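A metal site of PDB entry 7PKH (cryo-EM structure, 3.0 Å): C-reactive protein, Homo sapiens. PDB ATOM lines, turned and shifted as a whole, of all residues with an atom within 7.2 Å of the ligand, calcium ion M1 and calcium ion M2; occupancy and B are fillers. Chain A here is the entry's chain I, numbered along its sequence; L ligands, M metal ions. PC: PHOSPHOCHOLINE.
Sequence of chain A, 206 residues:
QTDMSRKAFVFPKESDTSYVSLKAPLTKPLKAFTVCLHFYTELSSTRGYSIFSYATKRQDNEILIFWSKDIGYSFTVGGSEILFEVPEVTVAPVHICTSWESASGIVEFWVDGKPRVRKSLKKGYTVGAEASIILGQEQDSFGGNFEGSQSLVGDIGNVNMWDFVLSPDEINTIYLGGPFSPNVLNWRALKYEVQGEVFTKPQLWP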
ATOM      1  N   TYR A  49      -9.483  11.908 -26.331  1.00  0.00           N
ATOM      2  CA  TYR A  49      -9.673  13.049 -25.457  1.00  0.00           C
ATOM      3  C   TYR A  49     -10.975  13.738 -25.800  1.00  0.00           C
ATOM      4  O   TYR A  49     -11.386  13.782 -26.961  1.00  0.00           O
ATOM      5  CB  TYR A  49      -8.469  13.999 -25.537  1.00  0.00           C
ATOM      6  CG  TYR A  49      -8.134  14.426 -26.943  1.00  0.00           C
ATOM      7  CD1 TYR A  49      -7.250  13.686 -27.696  1.00  0.00           C
ATOM      8  CD2 TYR A  49      -8.689  15.549 -27.518  1.00  0.00           C
ATOM      9  CE1 TYR A  49      -6.924  14.054 -28.965  1.00  0.00           C
ATOM     10  CE2 TYR A  49      -8.379  15.923 -28.788  1.00  0.00           C
ATOM     11  CZ  TYR A  49      -7.496  15.167 -29.512  1.00  0.00           C
ATOM     12  OH  TYR A  49      -7.178  15.511 -30.795  1.00  0.00           O
ATOM     13  N   SER A  50     -11.645  14.255 -24.770  1.00  0.00           N
ATOM     14  CA  SER A  50     -12.779  15.138 -24.959  1.00  0.00           C
ATOM     15  C   SER A  50     -12.366  16.496 -25.489  1.00  0.00           C
ATOM     16  O   SER A  50     -11.504  17.160 -24.919  1.00  0.00           O
ATOM     17  CB  SER A  50     -13.519  15.313 -23.636  1.00  0.00           C
ATOM     18  OG  SER A  50     -14.740  15.988 -23.841  1.00  0.00           O
ATOM     19  N   SER A  53     -17.537  18.817 -24.216  1.00  0.00           N
ATOM     20  CA  SER A  53     -18.499  17.985 -23.509  1.00  0.00           C
ATOM     21  C   SER A  53     -19.655  18.840 -23.017  1.00  0.00           C
ATOM     22  O   SER A  53     -19.452  19.767 -22.223  1.00  0.00           O
ATOM     23  CB  SER A  53     -17.833  17.275 -22.330  1.00  0.00           C
ATOM     24  OG  SER A  53     -18.804  16.613 -21.545  1.00  0.00           O
ATOM     25  N   ALA A  55     -23.348  18.302 -21.149  1.00  0.00           N
ATOM     26  CA  ALA A  55     -24.169  17.354 -20.413  1.00  0.00           C
ATOM     27  C   ALA A  55     -25.419  17.993 -19.845  1.00  0.00           C
ATOM     28  O   ALA A  55     -25.465  19.199 -19.592  1.00  0.00           O
ATOM     29  CB  ALA A  55     -23.420  16.700 -19.247  1.00  0.00           C
ATOM     30  N   GLN A  59     -28.516  13.220 -19.138  1.00  0.00           N
ATOM     31  CA  GLN A  59     -27.696  12.699 -20.233  1.00  0.00           C
ATOM     32  C   GLN A  59     -26.328  13.375 -20.171  1.00  0.00           C
ATOM     33  O   GLN A  59     -26.233  14.592 -20.374  1.00  0.00           O
ATOM     34  CB  GLN A  59     -28.378  12.942 -21.566  1.00  0.00           C
ATOM     35  CG  GLN A  59     -27.587  12.533 -22.779  1.00  0.00           C
ATOM     36  CD  GLN A  59     -27.265  11.068 -22.788  1.00  0.00           C
ATOM     37  OE1 GLN A  59     -26.795  10.503 -21.804  1.00  0.00           O
ATOM     38  NE2 GLN A  59     -27.548  10.419 -23.914  1.00  0.00           N
ATOM     39  N   ASP A  60     -25.299  12.589 -19.883  1.00  0.00           N
ATOM     40  CA  ASP A  60     -23.945  13.128 -19.781  1.00  0.00           C
ATOM     41  C   ASP A  60     -23.351  13.443 -21.146  1.00  0.00           C
ATOM     42  O   ASP A  60     -22.518  14.350 -21.258  1.00  0.00           O
ATOM     43  CB  ASP A  60     -23.059  12.140 -19.031  1.00  0.00           C
ATOM     44  CG  ASP A  60     -23.001  10.781 -19.703  1.00  0.00           C
ATOM     45  OD1 ASP A  60     -24.060  10.313 -20.173  1.00  0.00           O
ATOM     46  OD2 ASP A  60     -21.913  10.179 -19.767  1.00  0.00           O
ATOM     47  N   ASN A  61     -23.768  12.741 -22.190  1.00  0.00           N
ATOM     48  CA  ASN A  61     -23.233  12.931 -23.524  1.00  0.00           C
ATOM     49  C   ASN A  61     -24.239  13.620 -24.424  1.00  0.00           C
ATOM     50  O   ASN A  61     -24.480  13.190 -25.556  1.00  0.00           O
ATOM     51  CB  ASN A  61     -22.801  11.594 -24.128  1.00  0.00           C
ATOM     52  CG  ASN A  61     -21.659  10.956 -23.368  1.00  0.00           C
ATOM     53  OD1 ASN A  61     -21.508  11.165 -22.167  1.00  0.00           O
ATOM     54  ND2 ASN A  61     -20.851  10.184 -24.065  1.00  0.00           N
ATOM     55  N   LEU A  64     -21.327  15.632 -27.502  1.00  0.00           N
ATOM     56  CA  LEU A  64     -19.915  15.365 -27.291  1.00  0.00           C
ATOM     57  C   LEU A  64     -19.173  15.397 -28.621  1.00  0.00           C
ATOM     58  O   LEU A  64     -19.574  14.704 -29.558  1.00  0.00           O
ATOM     59  CB  LEU A  64     -19.709  14.024 -26.593  1.00  0.00           C
ATOM     60  CG  LEU A  64     -18.306  13.803 -26.073  1.00  0.00           C
ATOM     61  CD1 LEU A  64     -18.014  14.791 -24.980  1.00  0.00           C
ATOM     62  CD2 LEU A  64     -18.188  12.398 -25.566  1.00  0.00           C
ATOM     63  N   ILE A  65     -18.110  16.181 -28.685  1.00  0.00           N
ATOM     64  CA  ILE A  65     -17.093  16.042 -29.731  1.00  0.00           C
ATOM     65  C   ILE A  65     -15.873  15.381 -29.123  1.00  0.00           C
ATOM     66  O   ILE A  65     -15.282  15.905 -28.167  1.00  0.00           O
ATOM     67  CB  ILE A  65     -16.737  17.397 -30.369  1.00  0.00           C
ATOM     68  CG1 ILE A  65     -17.990  18.257 -30.567  1.00  0.00           C
ATOM     69  CG2 ILE A  65     -16.055  17.164 -31.705  1.00  0.00           C
ATOM     70  CD1 ILE A  65     -17.664  19.687 -30.905  1.00  0.00           C
ATOM     71  N   PHE A  66     -15.494  14.226 -29.657  1.00  0.00           N
ATOM     72  CA  PHE A  66     -14.488  13.364 -29.064  1.00  0.00           C
ATOM     73  C   PHE A  66     -13.530  12.872 -30.141  1.00  0.00           C
ATOM     74  O   PHE A  66     -13.973  12.417 -31.201  1.00  0.00           O
ATOM     75  CB  PHE A  66     -15.158  12.182 -28.364  1.00  0.00           C
ATOM     76  CG  PHE A  66     -14.341  11.571 -27.282  1.00  0.00           C
ATOM     77  CD1 PHE A  66     -14.428  12.016 -25.984  1.00  0.00           C
ATOM     78  CD2 PHE A  66     -13.488  10.518 -27.564  1.00  0.00           C
ATOM     79  CE1 PHE A  66     -13.673  11.460 -24.991  1.00  0.00           C
ATOM     80  CE2 PHE A  66     -12.724   9.950 -26.571  1.00  0.00           C
ATOM     81  CZ  PHE A  66     -12.827  10.418 -25.288  1.00  0.00           C
ATOM     82  N   TRP A  67     -12.235  12.984 -29.870  1.00  0.00           N
ATOM     83  CA  TRP A  67     -11.224  12.254 -30.625  1.00  0.00           C
ATOM     84  C   TRP A  67     -11.102  10.826 -30.111  1.00  0.00           C
ATOM     85  O   TRP A  67     -10.754  10.609 -28.952  1.00  0.00           O
ATOM     86  CB  TRP A  67      -9.864  12.941 -30.549  1.00  0.00           C
ATOM     87  CG  TRP A  67      -8.871  12.220 -31.398  1.00  0.00           C
ATOM     88  CD1 TRP A  67      -8.035  11.237 -31.011  1.00  0.00           C
ATOM     89  CD2 TRP A  67      -8.693  12.365 -32.813  1.00  0.00           C
ATOM     90  NE1 TRP A  67      -7.289  10.788 -32.068  1.00  0.00           N
ATOM     91  CE2 TRP A  67      -7.688  11.463 -33.195  1.00  0.00           C
ATOM     92  CE3 TRP A  67      -9.271  13.174 -33.788  1.00  0.00           C
ATOM     93  CZ2 TRP A  67      -7.254  11.343 -34.508  1.00  0.00           C
ATOM     94  CZ3 TRP A  67      -8.838  13.055 -35.086  1.00  0.00           C
ATOM     95  CH2 TRP A  67      -7.834  12.154 -35.440  1.00  0.00           C
ATOM     96  N   SER A  68     -11.385   9.857 -30.977  1.00  0.00           N
ATOM     97  CA  SER A  68     -11.286   8.446 -30.641  1.00  0.00           C
ATOM     98  C   SER A  68     -10.068   7.855 -31.331  1.00  0.00           C
ATOM     99  O   SER A  68      -9.959   7.921 -32.554  1.00  0.00           O
ATOM    100  CB  SER A  68     -12.546   7.688 -31.051  1.00  0.00           C
ATOM    101  OG  SER A  68     -13.669   8.141 -30.324  1.00  0.00           O
ATOM    102  N   SER A  74     -15.256  11.339 -33.151  1.00  0.00           N
ATOM    103  CA  SER A  74     -16.572  10.916 -32.725  1.00  0.00           C
ATOM    104  C   SER A  74     -17.435  12.141 -32.485  1.00  0.00           C
ATOM    105  O   SER A  74     -16.972  13.117 -31.867  1.00  0.00           O
ATOM    106  CB  SER A  74     -16.478  10.064 -31.467  1.00  0.00           C
ATOM    107  OG  SER A  74     -17.729   9.984 -30.817  1.00  0.00           O
ATOM    108  N   THR A  76     -21.354  12.846 -30.972  1.00  0.00           N
ATOM    109  CA  THR A  76     -22.550  12.284 -30.389  1.00  0.00           C
ATOM    110  C   THR A  76     -23.536  13.386 -30.056  1.00  0.00           C
ATOM    111  O   THR A  76     -23.147  14.488 -29.658  1.00  0.00           O
ATOM    112  CB  THR A  76     -22.248  11.535 -29.092  1.00  0.00           C
ATOM    113  OG1 THR A  76     -21.748  12.454 -28.118  1.00  0.00           O
ATOM    114  CG2 THR A  76     -21.188  10.500 -29.319  1.00  0.00           C
ATOM    115  N   GLU A  81     -23.959   8.026 -31.458  1.00  0.00           N
ATOM    116  CA  GLU A  81     -22.644   8.399 -31.974  1.00  0.00           C
ATOM    117  C   GLU A  81     -22.545   8.166 -33.470  1.00  0.00           C
ATOM    118  O   GLU A  81     -23.079   7.188 -33.998  1.00  0.00           O
ATOM    119  CB  GLU A  81     -21.555   7.592 -31.273  1.00  0.00           C
ATOM    120  CG  GLU A  81     -20.149   7.939 -31.693  1.00  0.00           C
ATOM    121  CD  GLU A  81     -19.118   7.110 -30.965  1.00  0.00           C
ATOM    122  OE1 GLU A  81     -19.508   6.259 -30.148  1.00  0.00           O
ATOM    123  OE2 GLU A  81     -17.916   7.309 -31.217  1.00  0.00           O
ATOM    124  N   GLU A 138     -13.995  15.047 -19.997  1.00  0.00           N
ATOM    125  CA  GLU A 138     -15.269  14.432 -20.292  1.00  0.00           C
ATOM    126  C   GLU A 138     -16.024  14.138 -19.017  1.00  0.00           C
ATOM    127  O   GLU A 138     -15.504  13.500 -18.100  1.00  0.00           O
ATOM    128  CB  GLU A 138     -15.068  13.114 -21.060  1.00  0.00           C
ATOM    129  CG  GLU A 138     -16.306  12.196 -21.074  1.00  0.00           C
ATOM    130  CD  GLU A 138     -17.255  12.525 -22.178  1.00  0.00           C
ATOM    131  OE1 GLU A 138     -16.793  13.116 -23.161  1.00  0.00           O
ATOM    132  OE2 GLU A 138     -18.455  12.236 -22.036  1.00  0.00           O
ATOM    133  N   GLN A 139     -17.264  14.609 -18.960  1.00  0.00           N
ATOM    134  CA  GLN A 139     -18.123  14.432 -17.814  1.00  0.00           C
ATOM    135  C   GLN A 139     -19.135  13.332 -18.027  1.00  0.00           C
ATOM    136  O   GLN A 139     -19.714  13.196 -19.102  1.00  0.00           O
ATOM    137  CB  GLN A 139     -18.809  15.751 -17.472  1.00  0.00           C
ATOM    138  CG  GLN A 139     -19.877  16.162 -18.427  1.00  0.00           C
ATOM    139  CD  GLN A 139     -20.107  17.651 -18.367  1.00  0.00           C
ATOM    140  OE1 GLN A 139     -19.456  18.336 -17.592  1.00  0.00           O
ATOM    141  NE2 GLN A 139     -20.931  18.165 -19.247  1.00  0.00           N
ATOM    142  N   ASP A 140     -19.344  12.533 -16.979  1.00  0.00           N
ATOM    143  CA  ASP A 140     -20.272  11.415 -17.004  1.00  0.00           C
ATOM    144  C   ASP A 140     -21.436  11.645 -16.059  1.00  0.00           C
ATOM    145  O   ASP A 140     -22.357  10.830 -15.995  1.00  0.00           O
ATOM    146  CB  ASP A 140     -19.552  10.108 -16.665  1.00  0.00           C
ATOM    147  CG  ASP A 140     -18.325   9.892 -17.524  1.00  0.00           C
ATOM    148  OD1 ASP A 140     -18.316  10.383 -18.674  1.00  0.00           O
ATOM    149  OD2 ASP A 140     -17.377   9.205 -17.080  1.00  0.00           O
ATOM    150  N   SER A 141     -21.421  12.773 -15.341  1.00  0.00           N
ATOM    151  CA  SER A 141     -22.560  13.268 -14.588  1.00  0.00           C
ATOM    152  C   SER A 141     -22.644  14.761 -14.856  1.00  0.00           C
ATOM    153  O   SER A 141     -21.776  15.342 -15.514  1.00  0.00           O
ATOM    154  CB  SER A 141     -22.423  12.966 -13.100  1.00  0.00           C
ATOM    155  OG  SER A 141     -21.296  13.616 -12.542  1.00  0.00           O
ATOM    156  N   GLY A 144     -19.215  16.293 -13.356  1.00  0.00           N
ATOM    157  CA  GLY A 144     -18.191  15.527 -12.673  1.00  0.00           C
ATOM    158  C   GLY A 144     -18.066  14.142 -13.250  1.00  0.00           C
ATOM    159  O   GLY A 144     -18.431  13.891 -14.399  1.00  0.00           O
ATOM    160  N   ASN A 145     -17.541  13.235 -12.429  1.00  0.00           N
ATOM    161  CA  ASN A 145     -17.072  11.932 -12.877  1.00  0.00           C
ATOM    162  C   ASN A 145     -16.138  12.036 -14.076  1.00  0.00           C
ATOM    163  O   ASN A 145     -16.267  11.338 -15.074  1.00  0.00           O
ATOM    164  CB  ASN A 145     -18.254  11.025 -13.209  1.00  0.00           C
ATOM    165  CG  ASN A 145     -19.089  10.689 -11.992  1.00  0.00           C
ATOM    166  OD1 ASN A 145     -18.691  10.944 -10.870  1.00  0.00           O
ATOM    167  ND2 ASN A 145     -20.255  10.110 -12.221  1.00  0.00           N
ATOM    168  N   PHE A 146     -15.181  12.955 -13.971  1.00  0.00           N
ATOM    169  CA  PHE A 146     -14.202  13.133 -15.029  1.00  0.00           C
ATOM    170  C   PHE A 146     -13.227  11.955 -15.062  1.00  0.00           C
ATOM    171  O   PHE A 146     -12.984  11.294 -14.061  1.00  0.00           O
ATOM    172  CB  PHE A 146     -13.445  14.443 -14.839  1.00  0.00           C
ATOM    173  CG  PHE A 146     -14.329  15.630 -14.697  1.00  0.00           C
ATOM    174  CD1 PHE A 146     -15.208  15.979 -15.701  1.00  0.00           C
ATOM    175  CD2 PHE A 146     -14.282  16.409 -13.555  1.00  0.00           C
ATOM    176  CE1 PHE A 146     -16.036  17.067 -15.568  1.00  0.00           C
ATOM    177  CE2 PHE A 146     -15.093  17.508 -13.422  1.00  0.00           C
ATOM    178  CZ  PHE A 146     -15.968  17.834 -14.432  1.00  0.00           C
ATOM    179  N   GLU A 147     -12.668  11.705 -16.253  1.00  0.00           N
ATOM    180  CA  GLU A 147     -11.780  10.567 -16.482  1.00  0.00           C
ATOM    181  C   GLU A 147     -10.421  11.104 -16.924  1.00  0.00           C
ATOM    182  O   GLU A 147     -10.333  11.831 -17.924  1.00  0.00           O
ATOM    183  CB  GLU A 147     -12.338   9.628 -17.549  1.00  0.00           C
ATOM    184  CG  GLU A 147     -13.796   9.273 -17.392  1.00  0.00           C
ATOM    185  CD  GLU A 147     -14.115   7.877 -17.912  1.00  0.00           C
ATOM    186  OE1 GLU A 147     -13.209   7.208 -18.447  1.00  0.00           O
ATOM    187  OE2 GLU A 147     -15.282   7.454 -17.807  1.00  0.00           O
ATOM    188  N   GLN A 150      -9.450  10.566 -20.449  1.00  0.00           N
ATOM    189  CA  GLN A 150     -10.199  11.306 -21.455  1.00  0.00           C
ATOM    190  C   GLN A 150      -9.995  12.820 -21.396  1.00  0.00           C
ATOM    191  O   GLN A 150     -10.596  13.537 -22.198  1.00  0.00           O
ATOM    192  CB  GLN A 150     -11.687  10.978 -21.371  1.00  0.00           C
ATOM    193  CG  GLN A 150     -11.940   9.502 -21.525  1.00  0.00           C
ATOM    194  CD  GLN A 150     -13.402   9.153 -21.510  1.00  0.00           C
ATOM    195  OE1 GLN A 150     -14.225   9.913 -21.004  1.00  0.00           O
ATOM    196  NE2 GLN A 150     -13.735   7.988 -22.038  1.00  0.00           N
HETATM  197  P1   PC L   1     -18.419   8.385 -21.460  1.00  0.00           P
HETATM  198  O1   PC L   1     -17.092   7.538 -21.167  1.00  0.00           O
HETATM  199  O3   PC L   1     -19.250   8.500 -20.244  1.00  0.00           O
HETATM  200  O4   PC L   1     -18.020   9.869 -21.875  1.00  0.00           O
HETATM  201  O2   PC L   1     -19.302   7.723 -22.625  1.00  0.00           O
HETATM  202  C1   PC L   1     -18.510   7.295 -23.746  1.00  0.00           C
HETATM  203  C2   PC L   1     -17.519   8.346 -24.275  1.00  0.00           C
HETATM  204  N1   PC L   1     -16.741   7.921 -25.453  1.00  0.00           N
HETATM  205  C3   PC L   1     -15.920   9.041 -25.898  1.00  0.00           C
HETATM  206  C4   PC L   1     -17.587   7.503 -26.576  1.00  0.00           C
HETATM  207  C5   PC L   1     -15.843   6.815 -25.108  1.00  0.00           C
HETATM  208 CA    CA M   1     -16.280   9.471 -19.214  1.00  0.00          CA
HETATM  209 CA    CA M   2     -19.586  11.042 -20.501  1.00  0.00          CA
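OG of Ser 53 lies close to NE2 of Gln 139 (3.5 Å). The side-chain amide nitrogen of Gln 139 lies close to the backbone NH of Ala 55, 3.1 Å away. OD1 of Asp 60 sits close to OE1 of Gln 59, 3.2 Å away. The backbone NH (N) of Ser 50 sits at hydrogen-bond distance from the backbone carbonyl oxygen (O) of Gln 150. O of Phe 66 lies within hydrogen-bond range of N of Ser 74, at 2.6 Å.
Of the 24 residues printed, 5 come within 4 Å of calcium ion M2.
Calcium ion M1 is bound by OD1 of Asp 140 (2.3 Å), OD2 of Asp 140 (2.4 Å), OE2 of Glu 147 (2.7 Å), OE1 of Gln 150 (2.8 Å) and O1 of the ligand (2.9 Å). Calcium ion M1 has five donor atoms within binding distance.
Of the 24 residues printed, 4 come within 4 Å of calcium ion M1.
Residues that only touch the ligand: Phe 66 (3.3 Å). Within 4 Å of the ligand: Asp 60, Asn 61, Phe 66, Glu 138, Asp 140, Glu 147 and Gln 150. Along chain A the residues within 4 Å of the ligand span positions 60 to 150. The nearest printed residue that does not touch the ligand is Leu 64 (4.1 Å).
OE2 of Glu 138 is bound to calcium ion M2 (2.2 Å). OD1 of Asp 140 is bound to calcium ion M2 (2.3 Å). Calcium ion M2 is bound by O4 of the ligand (2.4 Å). The side-chain amide oxygen (OD1) of Asn 61 is bound to calcium ion M2 (2.5 Å). Calcium ion M2 is bound by O of Gln 139 (2.6 Å). Calcium ion M2 is bound by O3 of the ligand, at 2.6 Å. Calcium ion M2 is bound by OD2 of Asp 60 (2.6 Å). Calcium ion M2 has seven donor atoms within binding distance.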
